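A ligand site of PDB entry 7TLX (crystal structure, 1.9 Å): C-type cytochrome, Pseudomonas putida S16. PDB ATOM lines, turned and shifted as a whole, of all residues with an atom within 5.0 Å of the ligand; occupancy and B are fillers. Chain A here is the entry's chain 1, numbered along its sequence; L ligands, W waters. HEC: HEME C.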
ATOM      1  N   ILE A  14      -8.937   2.182 -16.003  1.00  0.00           N
ATOM      2  CA  ILE A  14      -8.060   3.318 -16.288  1.00  0.00           C
ATOM      3  C   ILE A  14      -8.414   4.563 -15.451  1.00  0.00           C
ATOM      4  O   ILE A  14      -7.568   5.440 -15.247  1.00  0.00           O
ATOM      5  CB  ILE A  14      -8.073   3.640 -17.795  1.00  0.00           C
ATOM      6  CG1 ILE A  14      -6.739   4.260 -18.194  1.00  0.00           C
ATOM      7  CG2 ILE A  14      -9.218   4.557 -18.152  1.00  0.00           C
ATOM      8  CD1 ILE A  14      -6.485   4.203 -19.677  1.00  0.00           C
ATOM      9  N   CYS A  15      -9.649   4.658 -14.966  1.00  0.00           N
ATOM     10  CA  CYS A  15     -10.051   5.804 -14.161  1.00  0.00           C
ATOM     11  C   CYS A  15      -9.819   5.598 -12.679  1.00  0.00           C
ATOM     12  O   CYS A  15      -9.835   6.575 -11.914  1.00  0.00           O
ATOM     13  CB  CYS A  15     -11.566   6.092 -14.354  1.00  0.00           C
ATOM     14  SG  CYS A  15     -12.211   5.712 -16.016  1.00  0.00           S
ATOM     15  N   CYS A  18      -6.981   7.374 -10.136  1.00  0.00           N
ATOM     16  CA  CYS A  18      -7.230   8.766  -9.781  1.00  0.00           C
ATOM     17  C   CYS A  18      -8.532   8.929  -9.007  1.00  0.00           C
ATOM     18  O   CYS A  18      -8.561   9.623  -7.989  1.00  0.00           O
ATOM     19  CB  CYS A  18      -7.250   9.634 -11.054  1.00  0.00           C
ATOM     20  SG  CYS A  18      -5.693   9.645 -11.904  1.00  0.00           S
ATOM     21  N   HIS A  19      -9.606   8.282  -9.466  1.00  0.00           N
ATOM     22  CA  HIS A  19     -10.964   8.482  -8.956  1.00  0.00           C
ATOM     23  C   HIS A  19     -11.330   7.389  -7.981  1.00  0.00           C
ATOM     24  O   HIS A  19     -10.856   6.255  -8.075  1.00  0.00           O
ATOM     25  CB  HIS A  19     -12.001   8.429 -10.078  1.00  0.00           C
ATOM     26  CG  HIS A  19     -11.990   9.614 -10.974  1.00  0.00           C
ATOM     27  ND1 HIS A  19     -12.734  10.748 -10.716  1.00  0.00           N
ATOM     28  CD2 HIS A  19     -11.351   9.834 -12.137  1.00  0.00           C
ATOM     29  CE1 HIS A  19     -12.556  11.621 -11.700  1.00  0.00           C
ATOM     30  NE2 HIS A  19     -11.707  11.092 -12.577  1.00  0.00           N
ATOM     31  N   ALA A  30      -6.539  11.239  -6.517  1.00  0.00           N
ATOM     32  CA  ALA A  30      -6.285  12.465  -7.255  1.00  0.00           C
ATOM     33  C   ALA A  30      -7.547  13.121  -7.798  1.00  0.00           C
ATOM     34  O   ALA A  30      -7.441  14.220  -8.361  1.00  0.00           O
ATOM     35  CB  ALA A  30      -5.308  12.195  -8.430  1.00  0.00           C
ATOM     36  N   ALA A  31      -8.727  12.520  -7.652  1.00  0.00           N
ATOM     37  CA  ALA A  31      -9.886  12.923  -8.440  1.00  0.00           C
ATOM     38  C   ALA A  31     -11.159  12.617  -7.652  1.00  0.00           C
ATOM     39  O   ALA A  31     -11.160  11.759  -6.767  1.00  0.00           O
ATOM     40  CB  ALA A  31      -9.894  12.171  -9.789  1.00  0.00           C
ATOM     41  N   PRO A  32     -12.263  13.269  -7.987  1.00  0.00           N
ATOM     42  CA  PRO A  32     -13.494  13.157  -7.186  1.00  0.00           C
ATOM     43  C   PRO A  32     -14.123  11.767  -7.236  1.00  0.00           C
ATOM     44  O   PRO A  32     -13.978  10.998  -8.193  1.00  0.00           O
ATOM     45  CB  PRO A  32     -14.431  14.191  -7.836  1.00  0.00           C
ATOM     46  CG  PRO A  32     -13.879  14.431  -9.227  1.00  0.00           C
ATOM     47  CD  PRO A  32     -12.380  14.303  -9.045  1.00  0.00           C
ATOM     48  N   LEU A  34     -16.782   9.300  -8.148  1.00  0.00           N
ATOM     49  CA  LEU A  34     -17.718   9.302  -9.278  1.00  0.00           C
ATOM     50  C   LEU A  34     -19.039   8.616  -8.958  1.00  0.00           C
ATOM     51  O   LEU A  34     -19.851   8.449  -9.852  1.00  0.00           O
ATOM     52  CB  LEU A  34     -17.105   8.610 -10.492  1.00  0.00           C
ATOM     53  CG  LEU A  34     -15.884   9.333 -11.094  1.00  0.00           C
ATOM     54  CD1 LEU A  34     -15.375   8.599 -12.385  1.00  0.00           C
ATOM     55  CD2 LEU A  34     -16.204  10.857 -11.363  1.00  0.00           C
ATOM     56  N   LEU A  37     -22.590  10.097 -10.377  1.00  0.00           N
ATOM     57  CA  LEU A  37     -22.144  11.027 -11.410  1.00  0.00           C
ATOM     58  C   LEU A  37     -23.255  11.394 -12.401  1.00  0.00           C
ATOM     59  O   LEU A  37     -23.372  12.550 -12.826  1.00  0.00           O
ATOM     60  CB  LEU A  37     -20.998  10.380 -12.170  1.00  0.00           C
ATOM     61  CG  LEU A  37     -20.487  11.114 -13.396  1.00  0.00           C
ATOM     62  CD1 LEU A  37     -19.839  12.430 -12.993  1.00  0.00           C
ATOM     63  CD2 LEU A  37     -19.495  10.190 -14.132  1.00  0.00           C
ATOM     64  N   ARG A  40     -25.329  14.684 -12.437  1.00  0.00           N
ATOM     65  CA  ARG A  40     -24.828  15.580 -11.403  1.00  0.00           C
ATOM     66  C   ARG A  40     -24.301  16.870 -12.028  1.00  0.00           C
ATOM     67  O   ARG A  40     -23.683  16.836 -13.093  1.00  0.00           O
ATOM     68  CB  ARG A  40     -23.678  14.877 -10.660  1.00  0.00           C
ATOM     69  CG  ARG A  40     -23.000  15.624  -9.536  1.00  0.00           C
ATOM     70  CD  ARG A  40     -22.213  14.621  -8.668  1.00  0.00           C
ATOM     71  NE  ARG A  40     -20.818  14.472  -9.081  1.00  0.00           N
ATOM     72  CZ  ARG A  40     -20.029  13.482  -8.709  1.00  0.00           C
ATOM     73  NH1 ARG A  40     -20.450  12.512  -7.899  1.00  0.00           N
ATOM     74  NH2 ARG A  40     -18.754  13.474  -9.118  1.00  0.00           N
ATOM     75  N   LYS A  41     -24.473  17.994 -11.341  1.00  0.00           N
ATOM     76  CA  LYS A  41     -23.881  19.238 -11.836  1.00  0.00           C
ATOM     77  C   LYS A  41     -22.355  19.134 -11.855  1.00  0.00           C
ATOM     78  O   LYS A  41     -21.731  18.607 -10.918  1.00  0.00           O
ATOM     79  CB  LYS A  41     -24.312  20.431 -10.972  1.00  0.00           C
ATOM     80  CG  LYS A  41     -23.868  21.763 -11.575  1.00  0.00           C
ATOM     81  CD  LYS A  41     -24.536  22.979 -10.918  1.00  0.00           C
ATOM     82  CE  LYS A  41     -25.968  23.147 -11.367  1.00  0.00           C
ATOM     83  NZ  LYS A  41     -26.478  24.495 -10.892  1.00  0.00           N
ATOM     84  N   VAL A  42     -21.757  19.632 -12.941  1.00  0.00           N
ATOM     85  CA  VAL A  42     -20.297  19.617 -13.060  1.00  0.00           C
ATOM     86  C   VAL A  42     -19.658  20.348 -11.897  1.00  0.00           C
ATOM     87  O   VAL A  42     -20.128  21.411 -11.492  1.00  0.00           O
ATOM     88  CB  VAL A  42     -19.892  20.245 -14.398  1.00  0.00           C
ATOM     89  CG1 VAL A  42     -18.308  20.483 -14.481  1.00  0.00           C
ATOM     90  CG2 VAL A  42     -20.360  19.358 -15.533  1.00  0.00           C
ATOM     91  N   GLY A  43     -18.584  19.786 -11.345  1.00  0.00           N
ATOM     92  CA  GLY A  43     -17.735  20.470 -10.370  1.00  0.00           C
ATOM     93  C   GLY A  43     -18.499  20.900  -9.133  1.00  0.00           C
ATOM     94  O   GLY A  43     -18.332  22.020  -8.637  1.00  0.00           O
ATOM     95  N   SER A  44     -19.339  19.995  -8.600  1.00  0.00           N
ATOM     96  CA  SER A  44     -20.232  20.324  -7.502  1.00  0.00           C
ATOM     97  C   SER A  44     -20.190  19.331  -6.338  1.00  0.00           C
ATOM     98  O   SER A  44     -20.652  19.692  -5.247  1.00  0.00           O
ATOM     99  CB  SER A  44     -21.688  20.431  -7.999  1.00  0.00           C
ATOM    100  OG  SER A  44     -22.243  19.150  -8.331  1.00  0.00           O
ATOM    101  N   VAL A  45     -19.652  18.136  -6.516  1.00  0.00           N
ATOM    102  CA  VAL A  45     -19.664  17.159  -5.427  1.00  0.00           C
ATOM    103  C   VAL A  45     -18.831  17.717  -4.282  1.00  0.00           C
ATOM    104  O   VAL A  45     -17.748  18.283  -4.541  1.00  0.00           O
ATOM    105  CB  VAL A  45     -19.140  15.780  -5.918  1.00  0.00           C
ATOM    106  CG1 VAL A  45     -17.690  15.888  -6.396  1.00  0.00           C
ATOM    107  CG2 VAL A  45     -19.247  14.704  -4.793  1.00  0.00           C
ATOM    108  N   PHE A  48     -14.216  18.316  -2.926  1.00  0.00           N
ATOM    109  CA  PHE A  48     -13.149  18.197  -3.915  1.00  0.00           C
ATOM    110  C   PHE A  48     -12.856  19.582  -4.491  1.00  0.00           C
ATOM    111  O   PHE A  48     -13.775  20.313  -4.834  1.00  0.00           O
ATOM    112  CB  PHE A  48     -13.506  17.235  -5.046  1.00  0.00           C
ATOM    113  CG  PHE A  48     -12.350  17.008  -5.980  1.00  0.00           C
ATOM    114  CD1 PHE A  48     -11.336  16.119  -5.661  1.00  0.00           C
ATOM    115  CD2 PHE A  48     -12.220  17.802  -7.145  1.00  0.00           C
ATOM    116  CE1 PHE A  48     -10.226  15.943  -6.519  1.00  0.00           C
ATOM    117  CE2 PHE A  48     -11.123  17.671  -8.002  1.00  0.00           C
ATOM    118  CZ  PHE A  48     -10.106  16.738  -7.684  1.00  0.00           C
ATOM    119  N   LYS A  49     -11.571  19.930  -4.598  1.00  0.00           N
ATOM    120  CA  LYS A  49     -11.186  21.265  -5.062  1.00  0.00           C
ATOM    121  C   LYS A  49     -11.028  21.195  -6.579  1.00  0.00           C
ATOM    122  O   LYS A  49     -10.022  20.692  -7.078  1.00  0.00           O
ATOM    123  CB  LYS A  49      -9.915  21.753  -4.379  1.00  0.00           C
ATOM    124  CG  LYS A  49      -9.441  23.109  -4.913  1.00  0.00           C
ATOM    125  CD  LYS A  49      -8.863  24.022  -3.843  1.00  0.00           C
ATOM    126  CE  LYS A  49      -7.357  24.178  -3.985  1.00  0.00           C
ATOM    127  NZ  LYS A  49      -6.863  25.361  -3.217  1.00  0.00           N
ATOM    128  N   PHE A  50     -12.052  21.648  -7.293  1.00  0.00           N
ATOM    129  CA  PHE A  50     -12.025  21.620  -8.750  1.00  0.00           C
ATOM    130  C   PHE A  50     -11.203  22.764  -9.343  1.00  0.00           C
ATOM    131  O   PHE A  50     -10.968  23.788  -8.697  1.00  0.00           O
ATOM    132  CB  PHE A  50     -13.456  21.659  -9.300  1.00  0.00           C
ATOM    133  CG  PHE A  50     -14.215  20.354  -9.104  1.00  0.00           C
ATOM    134  CD1 PHE A  50     -14.088  19.331 -10.034  1.00  0.00           C
ATOM    135  CD2 PHE A  50     -15.077  20.177  -8.014  1.00  0.00           C
ATOM    136  CE1 PHE A  50     -14.780  18.130  -9.856  1.00  0.00           C
ATOM    137  CE2 PHE A  50     -15.777  18.991  -7.836  1.00  0.00           C
ATOM    138  CZ  PHE A  50     -15.627  17.972  -8.747  1.00  0.00           C
ATOM    139  N   SER A  51     -10.757  22.585 -10.594  1.00  0.00           N
ATOM    140  CA  SER A  51     -10.191  23.683 -11.366  1.00  0.00           C
ATOM    141  C   SER A  51     -11.244  24.765 -11.552  1.00  0.00           C
ATOM    142  O   SER A  51     -12.441  24.517 -11.422  1.00  0.00           O
ATOM    143  CB  SER A  51      -9.711  23.197 -12.737  1.00  0.00           C
ATOM    144  OG  SER A  51     -10.810  22.839 -13.560  1.00  0.00           O
ATOM    145  N   LEU A  54     -14.196  23.873 -13.968  1.00  0.00           N
ATOM    146  CA  LEU A  54     -15.264  23.025 -13.480  1.00  0.00           C
ATOM    147  C   LEU A  54     -15.939  23.649 -12.268  1.00  0.00           C
ATOM    148  O   LEU A  54     -17.159  23.505 -12.135  1.00  0.00           O
ATOM    149  CB  LEU A  54     -14.723  21.638 -13.142  1.00  0.00           C
ATOM    150  CG  LEU A  54     -14.657  20.695 -14.350  1.00  0.00           C
ATOM    151  CD1 LEU A  54     -13.579  21.125 -15.270  1.00  0.00           C
ATOM    152  CD2 LEU A  54     -14.400  19.245 -13.883  1.00  0.00           C
ATOM    153  N   TRP A  61     -23.641  16.739 -15.949  1.00  0.00           N
ATOM    154  CA  TRP A  61     -23.058  15.537 -16.556  1.00  0.00           C
ATOM    155  C   TRP A  61     -24.179  14.682 -17.170  1.00  0.00           C
ATOM    156  O   TRP A  61     -24.546  13.631 -16.663  1.00  0.00           O
ATOM    157  CB  TRP A  61     -22.233  14.757 -15.533  1.00  0.00           C
ATOM    158  CG  TRP A  61     -20.901  15.399 -15.272  1.00  0.00           C
ATOM    159  CD1 TRP A  61     -20.396  15.837 -14.059  1.00  0.00           C
ATOM    160  CD2 TRP A  61     -19.900  15.698 -16.258  1.00  0.00           C
ATOM    161  NE1 TRP A  61     -19.127  16.381 -14.241  1.00  0.00           N
ATOM    162  CE2 TRP A  61     -18.813  16.308 -15.580  1.00  0.00           C
ATOM    163  CE3 TRP A  61     -19.819  15.526 -17.643  1.00  0.00           C
ATOM    164  CZ2 TRP A  61     -17.652  16.747 -16.258  1.00  0.00           C
ATOM    165  CZ3 TRP A  61     -18.650  15.949 -18.322  1.00  0.00           C
ATOM    166  CH2 TRP A  61     -17.586  16.535 -17.628  1.00  0.00           C
ATOM    167  N   LEU A  66     -20.902  13.917 -20.907  1.00  0.00           N
ATOM    168  CA  LEU A  66     -19.869  13.003 -20.427  1.00  0.00           C
ATOM    169  C   LEU A  66     -19.134  12.349 -21.594  1.00  0.00           C
ATOM    170  O   LEU A  66     -17.895  12.196 -21.554  1.00  0.00           O
ATOM    171  CB  LEU A  66     -20.528  11.920 -19.591  1.00  0.00           C
ATOM    172  CG  LEU A  66     -20.603  12.134 -18.079  1.00  0.00           C
ATOM    173  CD1 LEU A  66     -21.627  11.194 -17.495  1.00  0.00           C
ATOM    174  CD2 LEU A  66     -19.221  11.889 -17.484  1.00  0.00           C
ATOM    175  N   PHE A  69     -16.645  14.846 -23.031  1.00  0.00           N
ATOM    176  CA  PHE A  69     -15.533  15.031 -22.097  1.00  0.00           C
ATOM    177  C   PHE A  69     -14.616  13.812 -22.072  1.00  0.00           C
ATOM    178  O   PHE A  69     -13.382  13.962 -22.057  1.00  0.00           O
ATOM    179  CB  PHE A  69     -16.084  15.313 -20.708  1.00  0.00           C
ATOM    180  CG  PHE A  69     -15.036  15.543 -19.649  1.00  0.00           C
ATOM    181  CD1 PHE A  69     -14.272  16.697 -19.613  1.00  0.00           C
ATOM    182  CD2 PHE A  69     -14.840  14.583 -18.654  1.00  0.00           C
ATOM    183  CE1 PHE A  69     -13.312  16.905 -18.596  1.00  0.00           C
ATOM    184  CE2 PHE A  69     -13.903  14.773 -17.628  1.00  0.00           C
ATOM    185  CZ  PHE A  69     -13.129  15.926 -17.593  1.00  0.00           C
ATOM    186  N   LEU A  70     -15.179  12.598 -22.026  1.00  0.00           N
ATOM    187  CA  LEU A  70     -14.296  11.428 -22.011  1.00  0.00           C
ATOM    188  C   LEU A  70     -13.537  11.264 -23.324  1.00  0.00           C
ATOM    189  O   LEU A  70     -12.482  10.618 -23.339  1.00  0.00           O
ATOM    190  CB  LEU A  70     -15.073  10.148 -21.722  1.00  0.00           C
ATOM    191  CG  LEU A  70     -15.616  10.078 -20.302  1.00  0.00           C
ATOM    192  CD1 LEU A  70     -16.051   8.651 -20.020  1.00  0.00           C
ATOM    193  CD2 LEU A  70     -14.578  10.539 -19.310  1.00  0.00           C
ATOM    194  N   LEU A  79      -8.866  24.042 -19.337  1.00  0.00           N
ATOM    195  CA  LEU A  79      -8.031  24.284 -18.182  1.00  0.00           C
ATOM    196  C   LEU A  79      -8.222  23.214 -17.100  1.00  0.00           C
ATOM    197  O   LEU A  79      -7.866  23.439 -15.942  1.00  0.00           O
ATOM    198  CB  LEU A  79      -8.293  25.701 -17.662  1.00  0.00           C
ATOM    199  CG  LEU A  79      -7.834  26.844 -18.595  1.00  0.00           C
ATOM    200  CD1 LEU A  79      -7.707  28.171 -17.866  1.00  0.00           C
ATOM    201  CD2 LEU A  79      -6.492  26.488 -19.247  1.00  0.00           C
ATOM    202  N   THR A  80      -8.741  22.042 -17.462  1.00  0.00           N
ATOM    203  CA  THR A  80      -9.015  20.999 -16.458  1.00  0.00           C
ATOM    204  C   THR A  80      -7.716  20.430 -15.882  1.00  0.00           C
ATOM    205  O   THR A  80      -6.668  20.400 -16.542  1.00  0.00           O
ATOM    206  CB  THR A  80      -9.846  19.847 -17.063  1.00  0.00           C
ATOM    207  OG1 THR A  80     -10.153  18.902 -16.034  1.00  0.00           O
ATOM    208  CG2 THR A  80      -9.080  19.110 -18.184  1.00  0.00           C
ATOM    209  N   ARG A  81      -7.797  19.965 -14.624  1.00  0.00           N
ATOM    210  CA  ARG A  81      -6.669  19.259 -14.015  1.00  0.00           C
ATOM    211  C   ARG A  81      -6.693  17.766 -14.278  1.00  0.00           C
ATOM    212  O   ARG A  81      -5.748  17.088 -13.851  1.00  0.00           O
ATOM    213  CB  ARG A  81      -6.614  19.460 -12.506  1.00  0.00           C
ATOM    214  CG  ARG A  81      -6.479  20.921 -12.067  1.00  0.00           C
ATOM    215  CD  ARG A  81      -5.276  21.625 -12.618  1.00  0.00           C
ATOM    216  NE  ARG A  81      -4.009  20.947 -12.339  1.00  0.00           N
ATOM    217  CZ  ARG A  81      -2.830  21.484 -12.620  1.00  0.00           C
ATOM    218  NH1 ARG A  81      -2.717  22.682 -13.169  1.00  0.00           N
ATOM    219  NH2 ARG A  81      -1.720  20.779 -12.349  1.00  0.00           N
ATOM    220  N   MET A  82      -7.734  17.235 -14.930  1.00  0.00           N
ATOM    221  CA  MET A  82      -7.740  15.839 -15.406  1.00  0.00           C
ATOM    222  C   MET A  82      -6.713  15.582 -16.493  1.00  0.00           C
ATOM    223  O   MET A  82      -6.945  15.939 -17.641  1.00  0.00           O
ATOM    224  CB  MET A  82      -9.118  15.425 -15.924  1.00  0.00           C
ATOM    225  CG  MET A  82      -9.238  13.912 -16.087  1.00  0.00           C
ATOM    226  SD  MET A  82     -10.943  13.407 -16.210  1.00  0.00           S
ATOM    227  CE  MET A  82     -10.900  12.167 -17.504  1.00  0.00           C
ATOM    228  N   ALA A  83      -5.612  14.901 -16.129  1.00  0.00           N
ATOM    229  CA  ALA A  83      -4.516  14.606 -17.052  1.00  0.00           C
ATOM    230  C   ALA A  83      -4.804  13.283 -17.760  1.00  0.00           C
ATOM    231  O   ALA A  83      -4.242  12.228 -17.441  1.00  0.00           O
ATOM    232  CB  ALA A  83      -3.185  14.540 -16.309  1.00  0.00           C
ATOM    233  N   PHE A  84      -5.690  13.335 -18.751  1.00  0.00           N
ATOM    234  CA  PHE A  84      -6.169  12.135 -19.421  1.00  0.00           C
ATOM    235  C   PHE A  84      -6.333  12.452 -20.901  1.00  0.00           C
ATOM    236  O   PHE A  84      -7.035  13.407 -21.259  1.00  0.00           O
ATOM    237  CB  PHE A  84      -7.510  11.682 -18.814  1.00  0.00           C
ATOM    238  CG  PHE A  84      -8.068  10.387 -19.400  1.00  0.00           C
ATOM    239  CD1 PHE A  84      -7.400   9.173 -19.206  1.00  0.00           C
ATOM    240  CD2 PHE A  84      -9.265  10.381 -20.105  1.00  0.00           C
ATOM    241  CE1 PHE A  84      -7.903   7.998 -19.739  1.00  0.00           C
ATOM    242  CE2 PHE A  84      -9.787   9.210 -20.622  1.00  0.00           C
ATOM    243  CZ  PHE A  84      -9.098   8.007 -20.443  1.00  0.00           C
ATOM    244  N   LEU A  87     -10.738   8.753 -24.239  1.00  0.00           N
ATOM    245  CA  LEU A  87     -11.063   7.443 -24.809  1.00  0.00           C
ATOM    246  C   LEU A  87     -11.522   7.671 -26.245  1.00  0.00           C
ATOM    247  O   LEU A  87     -12.617   8.187 -26.463  1.00  0.00           O
ATOM    248  CB  LEU A  87     -12.147   6.720 -24.013  1.00  0.00           C
ATOM    249  CG  LEU A  87     -11.961   6.471 -22.520  1.00  0.00           C
ATOM    250  CD1 LEU A  87     -13.288   6.087 -21.870  1.00  0.00           C
ATOM    251  CD2 LEU A  87     -10.910   5.383 -22.355  1.00  0.00           C
ATOM    252  N   VAL A  96     -18.074   2.433 -20.714  1.00  0.00           N
ATOM    253  CA  VAL A  96     -17.769   2.967 -19.391  1.00  0.00           C
ATOM    254  C   VAL A  96     -18.907   3.870 -18.913  1.00  0.00           C
ATOM    255  O   VAL A  96     -19.220   3.900 -17.716  1.00  0.00           O
ATOM    256  CB  VAL A  96     -16.413   3.684 -19.352  1.00  0.00           C
ATOM    257  CG1 VAL A  96     -16.495   5.049 -19.989  1.00  0.00           C
ATOM    258  CG2 VAL A  96     -15.948   3.821 -17.919  1.00  0.00           C
ATOM    259  N   LEU A 100     -21.009   3.440 -15.519  1.00  0.00           N
ATOM    260  CA  LEU A 100     -21.182   4.571 -14.612  1.00  0.00           C
ATOM    261  C   LEU A 100     -22.643   5.023 -14.467  1.00  0.00           C
ATOM    262  O   LEU A 100     -22.908   6.011 -13.782  1.00  0.00           O
ATOM    263  CB  LEU A 100     -20.326   5.739 -15.080  1.00  0.00           C
ATOM    264  CG  LEU A 100     -18.827   5.560 -14.792  1.00  0.00           C
ATOM    265  CD1 LEU A 100     -18.002   6.675 -15.414  1.00  0.00           C
ATOM    266  CD2 LEU A 100     -18.579   5.502 -13.288  1.00  0.00           C
HETATM  267 FE   HEC L   1     -11.271  12.080 -14.218  1.00  0.00          FE
HETATM  268  CHA HEC L   1     -12.665  15.007 -13.079  1.00  0.00           C
HETATM  269  CHB HEC L   1     -14.325  11.056 -15.287  1.00  0.00           C
HETATM  270  CHC HEC L   1      -9.796   9.290 -15.626  1.00  0.00           C
HETATM  271  CHD HEC L   1      -8.297  12.845 -12.763  1.00  0.00           C
HETATM  272  NA  HEC L   1     -13.131  12.896 -14.193  1.00  0.00           N
HETATM  273  C1A HEC L   1     -13.526  14.118 -13.679  1.00  0.00           C
HETATM  274  C2A HEC L   1     -14.958  14.301 -13.901  1.00  0.00           C
HETATM  275  C3A HEC L   1     -15.417  13.205 -14.536  1.00  0.00           C
HETATM  276  C4A HEC L   1     -14.273  12.316 -14.731  1.00  0.00           C
HETATM  277  CMA HEC L   1     -16.850  12.879 -15.026  1.00  0.00           C
HETATM  278  CAA HEC L   1     -15.775  15.518 -13.452  1.00  0.00           C
HETATM  279  CBA HEC L   1     -16.402  15.139 -12.093  1.00  0.00           C
HETATM  280  CGA HEC L   1     -17.371  16.159 -11.513  1.00  0.00           C
HETATM  281  O1A HEC L   1     -17.808  15.822 -10.382  1.00  0.00           O
HETATM  282  O2A HEC L   1     -17.609  17.198 -12.191  1.00  0.00           O
HETATM  283  NB  HEC L   1     -11.933  10.472 -15.226  1.00  0.00           N
HETATM  284  C1B HEC L   1     -13.251  10.207 -15.547  1.00  0.00           C
HETATM  285  C2B HEC L   1     -13.324   8.936 -16.216  1.00  0.00           C
HETATM  286  C3B HEC L   1     -12.066   8.466 -16.323  1.00  0.00           C
HETATM  287  C4B HEC L   1     -11.184   9.423 -15.710  1.00  0.00           C
HETATM  288  CMB HEC L   1     -14.661   8.308 -16.689  1.00  0.00           C
HETATM  289  CAB HEC L   1     -11.648   7.082 -16.983  1.00  0.00           C
HETATM  290  CBB HEC L   1     -12.046   6.956 -18.357  1.00  0.00           C
HETATM  291  NC  HEC L   1      -9.413  11.237 -14.216  1.00  0.00           N
HETATM  292  C1C HEC L   1      -8.996  10.089 -14.851  1.00  0.00           C
HETATM  293  C2C HEC L   1      -7.559   9.842 -14.567  1.00  0.00           C
HETATM  294  C3C HEC L   1      -7.161  10.847 -13.757  1.00  0.00           C
HETATM  295  C4C HEC L   1      -8.296  11.706 -13.521  1.00  0.00           C
HETATM  296  CMC HEC L   1      -6.744   8.660 -15.107  1.00  0.00           C
HETATM  297  CAC HEC L   1      -5.747  11.012 -13.062  1.00  0.00           C
HETATM  298  CBC HEC L   1      -4.633  11.035 -13.890  1.00  0.00           C
HETATM  299  ND  HEC L   1     -10.625  13.619 -13.154  1.00  0.00           N
HETATM  300  C1D HEC L   1      -9.311  13.778 -12.670  1.00  0.00           C
HETATM  301  C2D HEC L   1      -9.239  15.028 -11.981  1.00  0.00           C
HETATM  302  C3D HEC L   1     -10.451  15.620 -12.046  1.00  0.00           C
HETATM  303  C4D HEC L   1     -11.333  14.741 -12.793  1.00  0.00           C
HETATM  304  CMD HEC L   1      -7.943  15.541 -11.285  1.00  0.00           C
HETATM  305  CAD HEC L   1     -10.839  17.013 -11.530  1.00  0.00           C
HETATM  306  CBD HEC L   1     -10.620  17.993 -12.715  1.00  0.00           C
HETATM  307  CGD HEC L   1     -10.685  19.492 -12.550  1.00  0.00           C
HETATM  308  O1D HEC L   1     -10.987  19.950 -11.421  1.00  0.00           O
HETATM  309  O2D HEC L   1     -10.413  20.207 -13.558  1.00  0.00           O
HETATM  310  O   HOH W   1     -19.744  17.244  -9.485  1.00  0.00           O
HETATM  311  O   HOH W   2      -6.591   6.041 -12.943  1.00  0.00           O
HETATM  312  O   HOH W   3      -2.156  10.777 -16.343  1.00  0.00           O
HETATM  313  O   HOH W   4      -8.643  19.884  -9.498  1.00  0.00           O
HETATM  314  O   HOH W   5      -4.967  14.439 -13.356  1.00  0.00           O
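Water W4 bridges the backbone carbonyl oxygen of Lys 49 and an oxygen (O1D) of the ligand.
Merely in contact with the ligand: Ile 14 (3.3 Å), Ala 30 (3.2 Å), Ala 31 (3.3 Å), Pro 32 (3.8 Å), Leu 34 (3.9 Å), Leu 37 (3.6 Å), Val 42 (3.7 Å), Val 45 (3.99 Å), Phe 48 (3.6 Å), Phe 50 (3.3 Å), Leu 54 (3.7 Å), Leu 66 (3.6 Å), Phe 69 (3.8 Å), Leu 70 (3.4 Å), Ala 83 (3.8 Å), Phe 84 (3.8 Å), Leu 87 (3.8 Å) and Leu 100 (3.9 Å). Hydrophobic or aromatic side chains that line the ligand: Ile 14, His 19, Ala 31, Pro 32, Leu 34, Leu 37, Val 45, Phe 48, Phe 50, Leu 54, Trp 61, Leu 66, Phe 69, Leu 70, Met 82, Phe 84, Leu 87 and Leu 100. Within 4 Å of the ligand: Ile 14, Cys 15, Cys 18, His 19, Ala 30, Ala 31, Pro 32, Leu 34, Leu 37, Arg 40, Val 42, Gly 43, Val 45, Phe 48, Phe 50, Ser 51, Leu 54, Trp 61, Leu 66, Phe 69, Leu 70, Thr 80, Arg 81, Met 82, Ala 83, Phe 84, Leu 87 and Leu 100. The nearest printed residue that does not touch the ligand is Lys 49 (4.5 Å).
The side-chain hydroxyl (OG) of Ser 51 is in hydrogen-bond range of an oxygen (O2D) of the ligand (2.7 Å). The side-chain sulfur of Cys 18 is covalently linked to a carbon (CAC) of the ligand. N of Ser 51 lies within hydrogen-bond range of O1D of the ligand, at 2.8 Å. A carbon (CAB) of the ligand is bonded to the side-chain sulfur (SG) of Cys 15 (1.8 Å). An oxygen (O1A) of the ligand is in salt-bridge range of the guanidinium group (NH2) of Arg 40 (2.8 Å). O2A of the ligand is in hydrogen-bond range of NE1 of Trp 61, 2.7 Å away. O2D of the ligand lies within hydrogen-bond range of N of Arg 81 (2.8 Å). The backbone NH (N) of Gly 43 lies within hydrogen-bond range of an oxygen (O2A) of the ligand (2.9 Å). The side-chain sulfur (SD) of Met 82 binds an iron atom (FE) of the ligand, 2.4 Å away. OG1 of Thr 80 sits at hydrogen-bond distance from O2D of the ligand. A ring nitrogen (NE2) of His 19 binds an iron atom (FE) of the ligand.
The backbone NH (N) of Leu 87 lies within hydrogen-bond range of the backbone carbonyl oxygen (O) of Leu 70, 2.7 Å away. N of Ala 31 sits at hydrogen-bond distance from O of Cys 18, at 2.9 Å. N of Met 82 sits at hydrogen-bond distance from OG1 of Thr 80 (3.1 Å). N of Trp 61 lies within hydrogen-bond range of O of Arg 40, at 2.9 Å. The backbone carbonyl oxygen (O) of Cys 18 lies within hydrogen-bond range of the backbone NH (N) of Ala 30 (3.0 Å). The backbone carbonyl oxygen (O) of Pro 32 lies within hydrogen-bond range of a ring nitrogen (ND1) of His 19 (2.8 Å).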
